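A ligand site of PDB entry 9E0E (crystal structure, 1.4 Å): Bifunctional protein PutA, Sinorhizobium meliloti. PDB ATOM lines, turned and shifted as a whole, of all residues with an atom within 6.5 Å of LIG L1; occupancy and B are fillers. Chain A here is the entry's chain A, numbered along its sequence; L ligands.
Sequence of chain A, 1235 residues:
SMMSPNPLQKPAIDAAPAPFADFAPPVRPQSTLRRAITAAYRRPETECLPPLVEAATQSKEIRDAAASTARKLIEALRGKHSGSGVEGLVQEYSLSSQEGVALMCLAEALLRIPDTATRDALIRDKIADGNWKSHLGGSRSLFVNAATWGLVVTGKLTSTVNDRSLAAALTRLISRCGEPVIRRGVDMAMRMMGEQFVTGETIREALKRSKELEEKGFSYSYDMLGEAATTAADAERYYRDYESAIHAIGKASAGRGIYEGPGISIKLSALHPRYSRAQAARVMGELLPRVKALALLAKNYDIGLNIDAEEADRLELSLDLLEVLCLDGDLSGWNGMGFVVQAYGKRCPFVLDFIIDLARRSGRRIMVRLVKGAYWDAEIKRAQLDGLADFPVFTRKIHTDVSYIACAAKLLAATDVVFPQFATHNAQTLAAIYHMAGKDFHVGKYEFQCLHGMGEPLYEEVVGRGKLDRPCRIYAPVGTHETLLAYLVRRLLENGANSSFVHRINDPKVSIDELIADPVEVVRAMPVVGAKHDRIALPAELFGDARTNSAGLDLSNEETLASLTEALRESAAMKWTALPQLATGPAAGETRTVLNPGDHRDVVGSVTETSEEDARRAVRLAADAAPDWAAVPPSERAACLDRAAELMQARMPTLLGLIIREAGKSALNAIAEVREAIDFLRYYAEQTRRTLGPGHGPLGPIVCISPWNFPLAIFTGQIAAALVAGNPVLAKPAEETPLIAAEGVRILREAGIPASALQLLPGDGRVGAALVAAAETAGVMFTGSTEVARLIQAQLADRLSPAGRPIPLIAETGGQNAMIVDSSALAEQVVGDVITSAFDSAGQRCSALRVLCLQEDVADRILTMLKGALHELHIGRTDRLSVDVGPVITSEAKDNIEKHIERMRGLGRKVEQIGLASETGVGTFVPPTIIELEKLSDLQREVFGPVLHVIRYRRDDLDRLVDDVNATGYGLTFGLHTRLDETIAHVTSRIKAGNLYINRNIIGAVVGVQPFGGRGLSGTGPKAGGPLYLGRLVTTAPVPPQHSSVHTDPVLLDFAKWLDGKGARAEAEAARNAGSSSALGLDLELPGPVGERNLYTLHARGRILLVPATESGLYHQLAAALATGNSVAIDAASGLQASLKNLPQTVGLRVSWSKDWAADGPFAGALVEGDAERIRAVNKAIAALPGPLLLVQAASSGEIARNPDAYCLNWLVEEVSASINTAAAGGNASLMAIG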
ATOM      1  N   ASP A 223      -3.023 -18.980   4.296  1.00  0.00           N
ATOM      2  CA  ASP A 223      -2.741 -19.140   5.721  1.00  0.00           C
ATOM      3  C   ASP A 223      -1.666 -20.216   5.859  1.00  0.00           C
ATOM      4  O   ASP A 223      -1.921 -21.390   5.620  1.00  0.00           O
ATOM      5  CB  ASP A 223      -4.011 -19.554   6.449  1.00  0.00           C
ATOM      6  CG  ASP A 223      -3.739 -20.152   7.822  1.00  0.00           C
ATOM      7  OD1 ASP A 223      -2.837 -19.677   8.531  1.00  0.00           O
ATOM      8  OD2 ASP A 223      -4.473 -21.099   8.191  1.00  0.00           O
ATOM      9  N   GLU A 227       0.659 -20.589  14.396  1.00  0.00           N
ATOM     10  CA  GLU A 227      -0.232 -20.216  15.488  1.00  0.00           C
ATOM     11  C   GLU A 227       0.433 -20.577  16.806  1.00  0.00           C
ATOM     12  O   GLU A 227       1.112 -21.596  16.900  1.00  0.00           O
ATOM     13  CB  GLU A 227      -1.540 -20.998  15.347  1.00  0.00           C
ATOM     14  CG  GLU A 227      -2.575 -20.702  16.387  1.00  0.00           C
ATOM     15  CD  GLU A 227      -3.855 -21.435  16.072  1.00  0.00           C
ATOM     16  OE1 GLU A 227      -3.982 -21.918  14.920  1.00  0.00           O
ATOM     17  OE2 GLU A 227      -4.729 -21.528  16.960  1.00  0.00           O
ATOM     18  N   ILE A 266      -2.282 -13.726   8.637  1.00  0.00           N
ATOM     19  CA  ILE A 266      -1.308 -14.040   9.673  1.00  0.00           C
ATOM     20  C   ILE A 266      -2.012 -14.051  11.018  1.00  0.00           C
ATOM     21  O   ILE A 266      -3.075 -13.452  11.204  1.00  0.00           O
ATOM     22  CB  ILE A 266      -0.124 -13.054   9.716  1.00  0.00           C
ATOM     23  CG1 ILE A 266      -0.571 -11.658  10.154  1.00  0.00           C
ATOM     24  CG2 ILE A 266       0.577 -13.012   8.368  1.00  0.00           C
ATOM     25  CD1 ILE A 266       0.616 -10.734  10.451  1.00  0.00           C
ATOM     26  N   LYS A 267      -1.425 -14.775  11.970  1.00  0.00           N
ATOM     27  CA  LYS A 267      -1.882 -14.775  13.351  1.00  0.00           C
ATOM     28  C   LYS A 267      -0.796 -14.157  14.201  1.00  0.00           C
ATOM     29  O   LYS A 267       0.363 -14.582  14.147  1.00  0.00           O
ATOM     30  CB  LYS A 267      -2.175 -16.188  13.849  1.00  0.00           C
ATOM     31  CG  LYS A 267      -3.437 -16.791  13.262  1.00  0.00           C
ATOM     32  CD  LYS A 267      -3.588 -18.237  13.749  1.00  0.00           C
ATOM     33  CE  LYS A 267      -4.843 -18.886  13.209  1.00  0.00           C
ATOM     34  NZ  LYS A 267      -5.035 -18.616  11.749  1.00  0.00           N
ATOM     35  N   ASP A 308      -5.559 -12.179  11.470  1.00  0.00           N
ATOM     36  CA  ASP A 308      -6.645 -13.028  11.933  1.00  0.00           C
ATOM     37  C   ASP A 308      -6.963 -12.707  13.383  1.00  0.00           C
ATOM     38  O   ASP A 308      -6.114 -12.233  14.137  1.00  0.00           O
ATOM     39  CB  ASP A 308      -6.231 -14.506  11.858  1.00  0.00           C
ATOM     40  CG  ASP A 308      -6.281 -15.088  10.463  1.00  0.00           C
ATOM     41  OD1 ASP A 308      -6.668 -14.384   9.513  1.00  0.00           O
ATOM     42  OD2 ASP A 308      -5.936 -16.270  10.314  1.00  0.00           O
ATOM     43  N   ALA A 309      -8.200 -12.963  13.774  1.00  0.00           N
ATOM     44  CA  ALA A 309      -8.640 -12.729  15.151  1.00  0.00           C
ATOM     45  C   ALA A 309      -8.573 -14.015  15.943  1.00  0.00           C
ATOM     46  O   ALA A 309      -8.964 -15.083  15.461  1.00  0.00           O
ATOM     47  CB  ALA A 309     -10.061 -12.197  15.172  1.00  0.00           C
ATOM     48  N   GLU A 310      -8.084 -13.894  17.176  1.00  0.00           N
ATOM     49  CA  GLU A 310      -7.878 -15.079  17.997  1.00  0.00           C
ATOM     50  C   GLU A 310      -8.715 -14.984  19.267  1.00  0.00           C
ATOM     51  O   GLU A 310      -9.897 -14.638  19.199  1.00  0.00           O
ATOM     52  CB  GLU A 310      -6.388 -15.246  18.264  1.00  0.00           C
ATOM     53  CG  GLU A 310      -5.615 -15.367  16.948  1.00  0.00           C
ATOM     54  CD  GLU A 310      -4.137 -15.644  17.148  1.00  0.00           C
ATOM     55  OE1 GLU A 310      -3.804 -16.808  17.487  1.00  0.00           O
ATOM     56  OE2 GLU A 310      -3.321 -14.714  16.970  1.00  0.00           O
ATOM     57  N   GLN A 342     -14.781 -10.476  15.158  1.00  0.00           N
ATOM     58  CA  GLN A 342     -15.601 -11.656  15.414  1.00  0.00           C
ATOM     59  C   GLN A 342     -16.961 -11.220  15.912  1.00  0.00           C
ATOM     60  O   GLN A 342     -17.085 -10.668  17.016  1.00  0.00           O
ATOM     61  CB  GLN A 342     -14.906 -12.549  16.442  1.00  0.00           C
ATOM     62  CG  GLN A 342     -13.525 -13.014  15.980  1.00  0.00           C
ATOM     63  CD  GLN A 342     -12.583 -13.257  17.113  1.00  0.00           C
ATOM     64  OE1 GLN A 342     -12.401 -12.398  17.994  1.00  0.00           O
ATOM     65  NE2 GLN A 342     -11.944 -14.426  17.118  1.00  0.00           N
ATOM     66  N   ARG A 369     -12.413  -8.139   7.769  1.00  0.00           N
ATOM     67  CA  ARG A 369     -13.064  -9.425   7.605  1.00  0.00           C
ATOM     68  C   ARG A 369     -14.005  -9.643   8.774  1.00  0.00           C
ATOM     69  O   ARG A 369     -13.567  -9.711   9.928  1.00  0.00           O
ATOM     70  CB  ARG A 369     -12.047 -10.554   7.544  1.00  0.00           C
ATOM     71  CG  ARG A 369     -12.751 -11.884   7.288  1.00  0.00           C
ATOM     72  CD  ARG A 369     -11.868 -13.071   7.638  1.00  0.00           C
ATOM     73  NE  ARG A 369     -10.726 -13.155   6.743  1.00  0.00           N
ATOM     74  CZ  ARG A 369      -9.549 -13.652   7.085  1.00  0.00           C
ATOM     75  NH1 ARG A 369      -9.339 -14.187   8.282  1.00  0.00           N
ATOM     76  NH2 ARG A 369      -8.552 -13.605   6.206  1.00  0.00           N
ATOM     77  N   GLY A 373     -16.753 -16.374  14.558  1.00  0.00           N
ATOM     78  CA  GLY A 373     -15.723 -16.556  15.555  1.00  0.00           C
ATOM     79  C   GLY A 373     -15.417 -18.017  15.789  1.00  0.00           C
ATOM     80  O   GLY A 373     -16.335 -18.837  15.822  1.00  0.00           O
ATOM     81  N   ALA A 374     -14.153 -18.366  15.970  1.00  0.00           N
ATOM     82  CA  ALA A 374     -13.752 -19.766  15.928  1.00  0.00           C
ATOM     83  C   ALA A 374     -13.450 -20.373  17.285  1.00  0.00           C
ATOM     84  O   ALA A 374     -13.153 -21.577  17.348  1.00  0.00           O
ATOM     85  CB  ALA A 374     -12.515 -19.909  15.033  1.00  0.00           C
ATOM     86  N   TYR A 375     -13.536 -19.614  18.371  1.00  0.00           N
ATOM     87  CA  TYR A 375     -13.051 -20.068  19.673  1.00  0.00           C
ATOM     88  C   TYR A 375     -14.166 -20.159  20.702  1.00  0.00           C
ATOM     89  O   TYR A 375     -13.905 -20.030  21.901  1.00  0.00           O
ATOM     90  CB  TYR A 375     -11.960 -19.135  20.204  1.00  0.00           C
ATOM     91  CG  TYR A 375     -10.807 -18.948  19.261  1.00  0.00           C
ATOM     92  CD1 TYR A 375     -10.895 -18.071  18.187  1.00  0.00           C
ATOM     93  CD2 TYR A 375      -9.631 -19.649  19.438  1.00  0.00           C
ATOM     94  CE1 TYR A 375      -9.846 -17.898  17.305  1.00  0.00           C
ATOM     95  CE2 TYR A 375      -8.560 -19.487  18.584  1.00  0.00           C
ATOM     96  CZ  TYR A 375      -8.683 -18.617  17.518  1.00  0.00           C
ATOM     97  OH  TYR A 375      -7.612 -18.456  16.664  1.00  0.00           O
ATOM     98  N   HIS A 425     -20.111 -19.297   5.662  1.00  0.00           N
ATOM     99  CA  HIS A 425     -20.628 -20.389   4.853  1.00  0.00           C
ATOM    100  C   HIS A 425     -22.121 -20.524   4.971  1.00  0.00           C
ATOM    101  O   HIS A 425     -22.698 -21.457   4.400  1.00  0.00           O
ATOM    102  CB  HIS A 425     -19.957 -21.694   5.289  1.00  0.00           C
ATOM    103  CG  HIS A 425     -18.485 -21.689   5.082  1.00  0.00           C
ATOM    104  ND1 HIS A 425     -17.598 -22.178   6.016  1.00  0.00           N
ATOM    105  CD2 HIS A 425     -17.737 -21.196   4.072  1.00  0.00           C
ATOM    106  CE1 HIS A 425     -16.366 -22.019   5.566  1.00  0.00           C
ATOM    107  NE2 HIS A 425     -16.416 -21.421   4.387  1.00  0.00           N
ATOM    108  N   LEU A 451     -13.921 -20.652   3.268  1.00  0.00           N
ATOM    109  CA  LEU A 451     -12.775 -21.512   3.531  1.00  0.00           C
ATOM    110  C   LEU A 451     -12.594 -22.489   2.392  1.00  0.00           C
ATOM    111  O   LEU A 451     -13.565 -23.034   1.856  1.00  0.00           O
ATOM    112  CB  LEU A 451     -12.993 -22.282   4.838  1.00  0.00           C
ATOM    113  CG  LEU A 451     -11.930 -23.301   5.232  1.00  0.00           C
ATOM    114  CD1 LEU A 451     -10.574 -22.635   5.469  1.00  0.00           C
ATOM    115  CD2 LEU A 451     -12.402 -24.038   6.481  1.00  0.00           C
ATOM    116  N   TYR A 475     -10.067 -18.503   1.819  1.00  0.00           N
ATOM    117  CA  TYR A 475      -9.030 -18.635   2.835  1.00  0.00           C
ATOM    118  C   TYR A 475      -8.395 -20.004   2.658  1.00  0.00           C
ATOM    119  O   TYR A 475      -9.078 -21.033   2.765  1.00  0.00           O
ATOM    120  CB  TYR A 475      -9.677 -18.518   4.215  1.00  0.00           C
ATOM    121  CG  TYR A 475      -8.716 -18.442   5.369  1.00  0.00           C
ATOM    122  CD1 TYR A 475      -8.179 -19.592   5.936  1.00  0.00           C
ATOM    123  CD2 TYR A 475      -8.365 -17.206   5.917  1.00  0.00           C
ATOM    124  CE1 TYR A 475      -7.309 -19.516   7.021  1.00  0.00           C
ATOM    125  CE2 TYR A 475      -7.504 -17.131   6.998  1.00  0.00           C
ATOM    126  CZ  TYR A 475      -6.975 -18.282   7.536  1.00  0.00           C
ATOM    127  OH  TYR A 475      -6.118 -18.203   8.601  1.00  0.00           O
ATOM    128  N   ARG A 490     -10.611 -27.815  15.860  1.00  0.00           N
ATOM    129  CA  ARG A 490     -11.300 -26.527  15.935  1.00  0.00           C
ATOM    130  C   ARG A 490     -11.851 -26.115  14.571  1.00  0.00           C
ATOM    131  O   ARG A 490     -12.960 -25.576  14.483  1.00  0.00           O
ATOM    132  CB  ARG A 490     -10.349 -25.457  16.495  1.00  0.00           C
ATOM    133  CG  ARG A 490     -10.960 -24.060  16.636  1.00  0.00           C
ATOM    134  CD  ARG A 490      -9.878 -23.020  16.915  1.00  0.00           C
ATOM    135  NE  ARG A 490      -9.038 -22.776  15.745  1.00  0.00           N
ATOM    136  CZ  ARG A 490      -7.746 -22.494  15.787  1.00  0.00           C
ATOM    137  NH1 ARG A 490      -7.084 -22.470  16.932  1.00  0.00           N
ATOM    138  NH2 ARG A 490      -7.093 -22.235  14.659  1.00  0.00           N
ATOM    139  N   ARG A 491     -11.097 -26.392  13.513  1.00  0.00           N
ATOM    140  CA  ARG A 491     -11.513 -25.980  12.167  1.00  0.00           C
ATOM    141  C   ARG A 491     -12.759 -26.728  11.733  1.00  0.00           C
ATOM    142  O   ARG A 491     -13.647 -26.146  11.094  1.00  0.00           O
ATOM    143  CB  ARG A 491     -10.370 -26.195  11.184  1.00  0.00           C
ATOM    144  N   GLU A 494     -16.182 -25.665  13.381  1.00  0.00           N
ATOM    145  CA  GLU A 494     -16.759 -24.425  12.877  1.00  0.00           C
ATOM    146  C   GLU A 494     -17.921 -24.699  11.930  1.00  0.00           C
ATOM    147  O   GLU A 494     -19.009 -24.144  12.110  1.00  0.00           O
ATOM    148  CB  GLU A 494     -15.698 -23.580  12.177  1.00  0.00           C
HETATM  149  C1  LIG L   1      -7.846 -17.464  12.821  1.00  0.00           C
HETATM  150  C2  LIG L   1      -8.840 -18.394  12.146  1.00  0.00           C
HETATM  151  C3  LIG L   1      -8.969 -18.386  10.766  1.00  0.00           C
HETATM  152  C4  LIG L   1      -9.892 -19.249  10.135  1.00  0.00           C
HETATM  153  C5  LIG L   1     -10.667 -20.099  10.886  1.00  0.00           C
HETATM  154  C6  LIG L   1     -11.249 -20.450   8.795  1.00  0.00           C
HETATM  155  C7  LIG L   1     -10.276 -19.470   8.794  1.00  0.00           C
HETATM  156  C8  LIG L   1     -10.515 -20.119  12.294  1.00  0.00           C
HETATM  157  C9  LIG L   1      -9.611 -19.268  12.920  1.00  0.00           C
HETATM  158  N1  LIG L   1     -11.468 -20.824  10.045  1.00  0.00           N
HETATM  159  O1  LIG L   1      -8.014 -17.508  14.210  1.00  0.00           O
HETATM  160  P1  LG2 L   2     -22.529 -20.710  10.998  1.00  0.00           P
HETATM  161  O1  LG2 L   2     -22.928 -22.194  11.162  1.00  0.00           O
HETATM  162  O2  LG2 L   2     -23.511 -19.761  10.519  1.00  0.00           O
HETATM  163  O3  LG2 L   2     -22.016 -20.084  12.237  1.00  0.00           O
HETATM  164  C1  LG2 L   2     -21.325 -20.875  13.197  1.00  0.00           C
HETATM  165  C2  LG2 L   2     -20.750 -19.973  14.270  1.00  0.00           C
HETATM  166  O4  LG2 L   2     -21.724 -19.613  15.207  1.00  0.00           O
HETATM  167  C3  LG2 L   2     -19.648 -20.540  15.116  1.00  0.00           C
HETATM  168  O5  LG2 L   2     -18.424 -20.642  14.460  1.00  0.00           O
HETATM  169  C4  LG2 L   2     -19.620 -19.571  16.233  1.00  0.00           C
HETATM  170  O6  LG2 L   2     -18.982 -18.367  15.935  1.00  0.00           O
HETATM  171  C5  LG2 L   2     -21.066 -19.272  16.397  1.00  0.00           C
HETATM  172  N1  LG2 L   2     -21.725 -20.029  17.430  1.00  0.00           N
HETATM  173  C6  LG2 L   2     -21.953 -21.394  17.451  1.00  0.00           C
HETATM  174  N2  LG2 L   2     -22.599 -21.697  18.576  1.00  0.00           N
HETATM  175  C7  LG2 L   2     -22.824 -20.548  19.324  1.00  0.00           C
HETATM  176  C8  LG2 L   2     -23.423 -20.264  20.528  1.00  0.00           C
HETATM  177  N3  LG2 L   2     -24.027 -21.283  21.338  1.00  0.00           N
HETATM  178  N4  LG2 L   2     -23.465 -18.999  20.961  1.00  0.00           N
HETATM  179  C9  LG2 L   2     -22.928 -17.982  20.250  1.00  0.00           C
HETATM  180  N5  LG2 L   2     -22.330 -18.226  19.064  1.00  0.00           N
HETATM  181  C10 LG2 L   2     -22.265 -19.472  18.599  1.00  0.00           C
HETATM  182  N6  LG2 L   2     -12.638 -17.250  13.013  1.00  0.00           N
HETATM  183  C11 LG2 L   2     -11.951 -16.414  13.930  1.00  0.00           C
HETATM  184  O7  LG2 L   2     -12.250 -16.449  15.214  1.00  0.00           O
HETATM  185  N7  LG2 L   2     -10.896 -15.646  13.533  1.00  0.00           N
HETATM  186  C12 LG2 L   2     -10.555 -15.572  12.218  1.00  0.00           C
HETATM  187  O8  LG2 L   2      -9.521 -14.795  11.866  1.00  0.00           O
HETATM  188  C13 LG2 L   2     -11.377 -16.231  11.184  1.00  0.00           C
HETATM  189  N8  LG2 L   2     -11.174 -16.049   9.827  1.00  0.00           N
HETATM  190  C14 LG2 L   2     -12.041 -16.673   8.934  1.00  0.00           C
HETATM  191  C15 LG2 L   2     -11.884 -16.496   7.556  1.00  0.00           C
HETATM  192  C16 LG2 L   2     -12.738 -17.132   6.687  1.00  0.00           C
HETATM  193  C17 LG2 L   2     -12.552 -16.900   5.206  1.00  0.00           C
HETATM  194  C18 LG2 L   2     -13.752 -17.962   7.154  1.00  0.00           C
HETATM  195  C19 LG2 L   2     -14.674 -18.668   6.209  1.00  0.00           C
HETATM  196  C20 LG2 L   2     -13.906 -18.160   8.506  1.00  0.00           C
HETATM  197  C21 LG2 L   2     -13.047 -17.518   9.388  1.00  0.00           C
HETATM  198  N9  LG2 L   2     -13.246 -17.724  10.769  1.00  0.00           N
HETATM  199  C22 LG2 L   2     -12.409 -17.092  11.678  1.00  0.00           C
HETATM  200  C23 LG2 L   2     -14.279 -18.661  11.235  1.00  0.00           C
HETATM  201  C24 LG2 L   2     -15.600 -18.050  11.524  1.00  0.00           C
HETATM  202  O9  LG2 L   2     -15.372 -17.282  12.621  1.00  0.00           O
HETATM  203  C25 LG2 L   2     -16.611 -19.154  11.867  1.00  0.00           C
HETATM  204  O10 LG2 L   2     -16.147 -19.933  12.911  1.00  0.00           O
HETATM  205  C26 LG2 L   2     -16.972 -20.126  10.753  1.00  0.00           C
HETATM  206  O11 LG2 L   2     -16.762 -19.591   9.503  1.00  0.00           O
HETATM  207  C27 LG2 L   2     -18.427 -20.550  10.962  1.00  0.00           C
HETATM  208  O12 LG2 L   2     -19.346 -19.480  10.774  1.00  0.00           O
HETATM  209  P2  LG2 L   2     -20.307 -19.549   9.497  1.00  0.00           P
HETATM  210  O13 LG2 L   2     -19.577 -19.967   8.187  1.00  0.00           O
HETATM  211  O14 LG2 L   2     -21.056 -18.183   9.487  1.00  0.00           O
HETATM  212  O15 LG2 L   2     -21.462 -20.595   9.971  1.00  0.00           O
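N of Ala 309 is in hydrogen-bond range of O8 of LG2 L2 (3.0 Å).
The backbone NH of Ala 374 lies within hydrogen-bond range of an oxygen (O7) of LG2 L2.
An oxygen (O1) of LIG L1 is in hydrogen-bond range of the side-chain hydroxyl (OH) of Tyr 375, at 2.7 Å.
The backbone NH (N) of His 425 lies within hydrogen-bond range of an oxygen (O13) of LG2 L2 (2.7 Å).
O7 of LG2 L2 is in hydrogen-bond range of NE2 of Gln 342.
N of Gly 373 is in hydrogen-bond range of O9 of LG2 L2 (2.5 Å).
A nitrogen (N7) of LG2 L2 is in hydrogen-bond range of the backbone carbonyl oxygen (O) of Ala 309 (2.8 Å).
An oxygen (O1) of LIG L1 is in hydrogen-bond range of the backbone carbonyl oxygen of Ala 309 (2.9 Å).
The guanidinium group (NH1) of Arg 369 sits at hydrogen-bond distance from a nitrogen (N8) of LG2 L2 (3.0 Å).
O of Gly 373 lies within hydrogen-bond range of O6 of LG2 L2 (2.7 Å).
O1 of LIG L1 lies within hydrogen-bond range of N7 of LG2 L2 (3.5 Å).
The side-chain amide nitrogen of Gln 342 sits at hydrogen-bond distance from the backbone carbonyl oxygen of Ala 309, 3.5 Å away.
The side-chain amino group (NZ) of Lys 267 is in salt-bridge range of the side-chain carboxylate (OD2) of Asp 308 (2.9 Å).
The side-chain hydroxyl of Tyr 475 sits close to the side-chain carboxylate of Asp 223 (3.4 Å).
The side-chain carboxylate (OD2) of Asp 308 lies within hydrogen-bond range of the side-chain hydroxyl (OH) of Tyr 475, at 2.6 Å.
N of Asp 308 sits at hydrogen-bond distance from O of Ile 266 (2.8 Å).
OH of Tyr 475 is in hydrogen-bond range of NZ of Lys 267 (3.4 Å).
The side-chain carboxylate (OD1) of Asp 308 lies within salt-bridge range of the guanidinium group (NH1) of Arg 369.
NZ of Lys 267 touches C1 of LIG L1, 3.2 Å away.
Asp 308 touches LIG L1.
Ala 374 touches LIG L1.
Tyr 475 touches LIG L1.
Within 4 Å of LIG L1: Lys 267, Asp 308, Ala 309, Ala 374, Tyr 375 and Tyr 475.
The nearest printed residue that does not touch LIG L1 is Leu 451 (4.04 Å).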
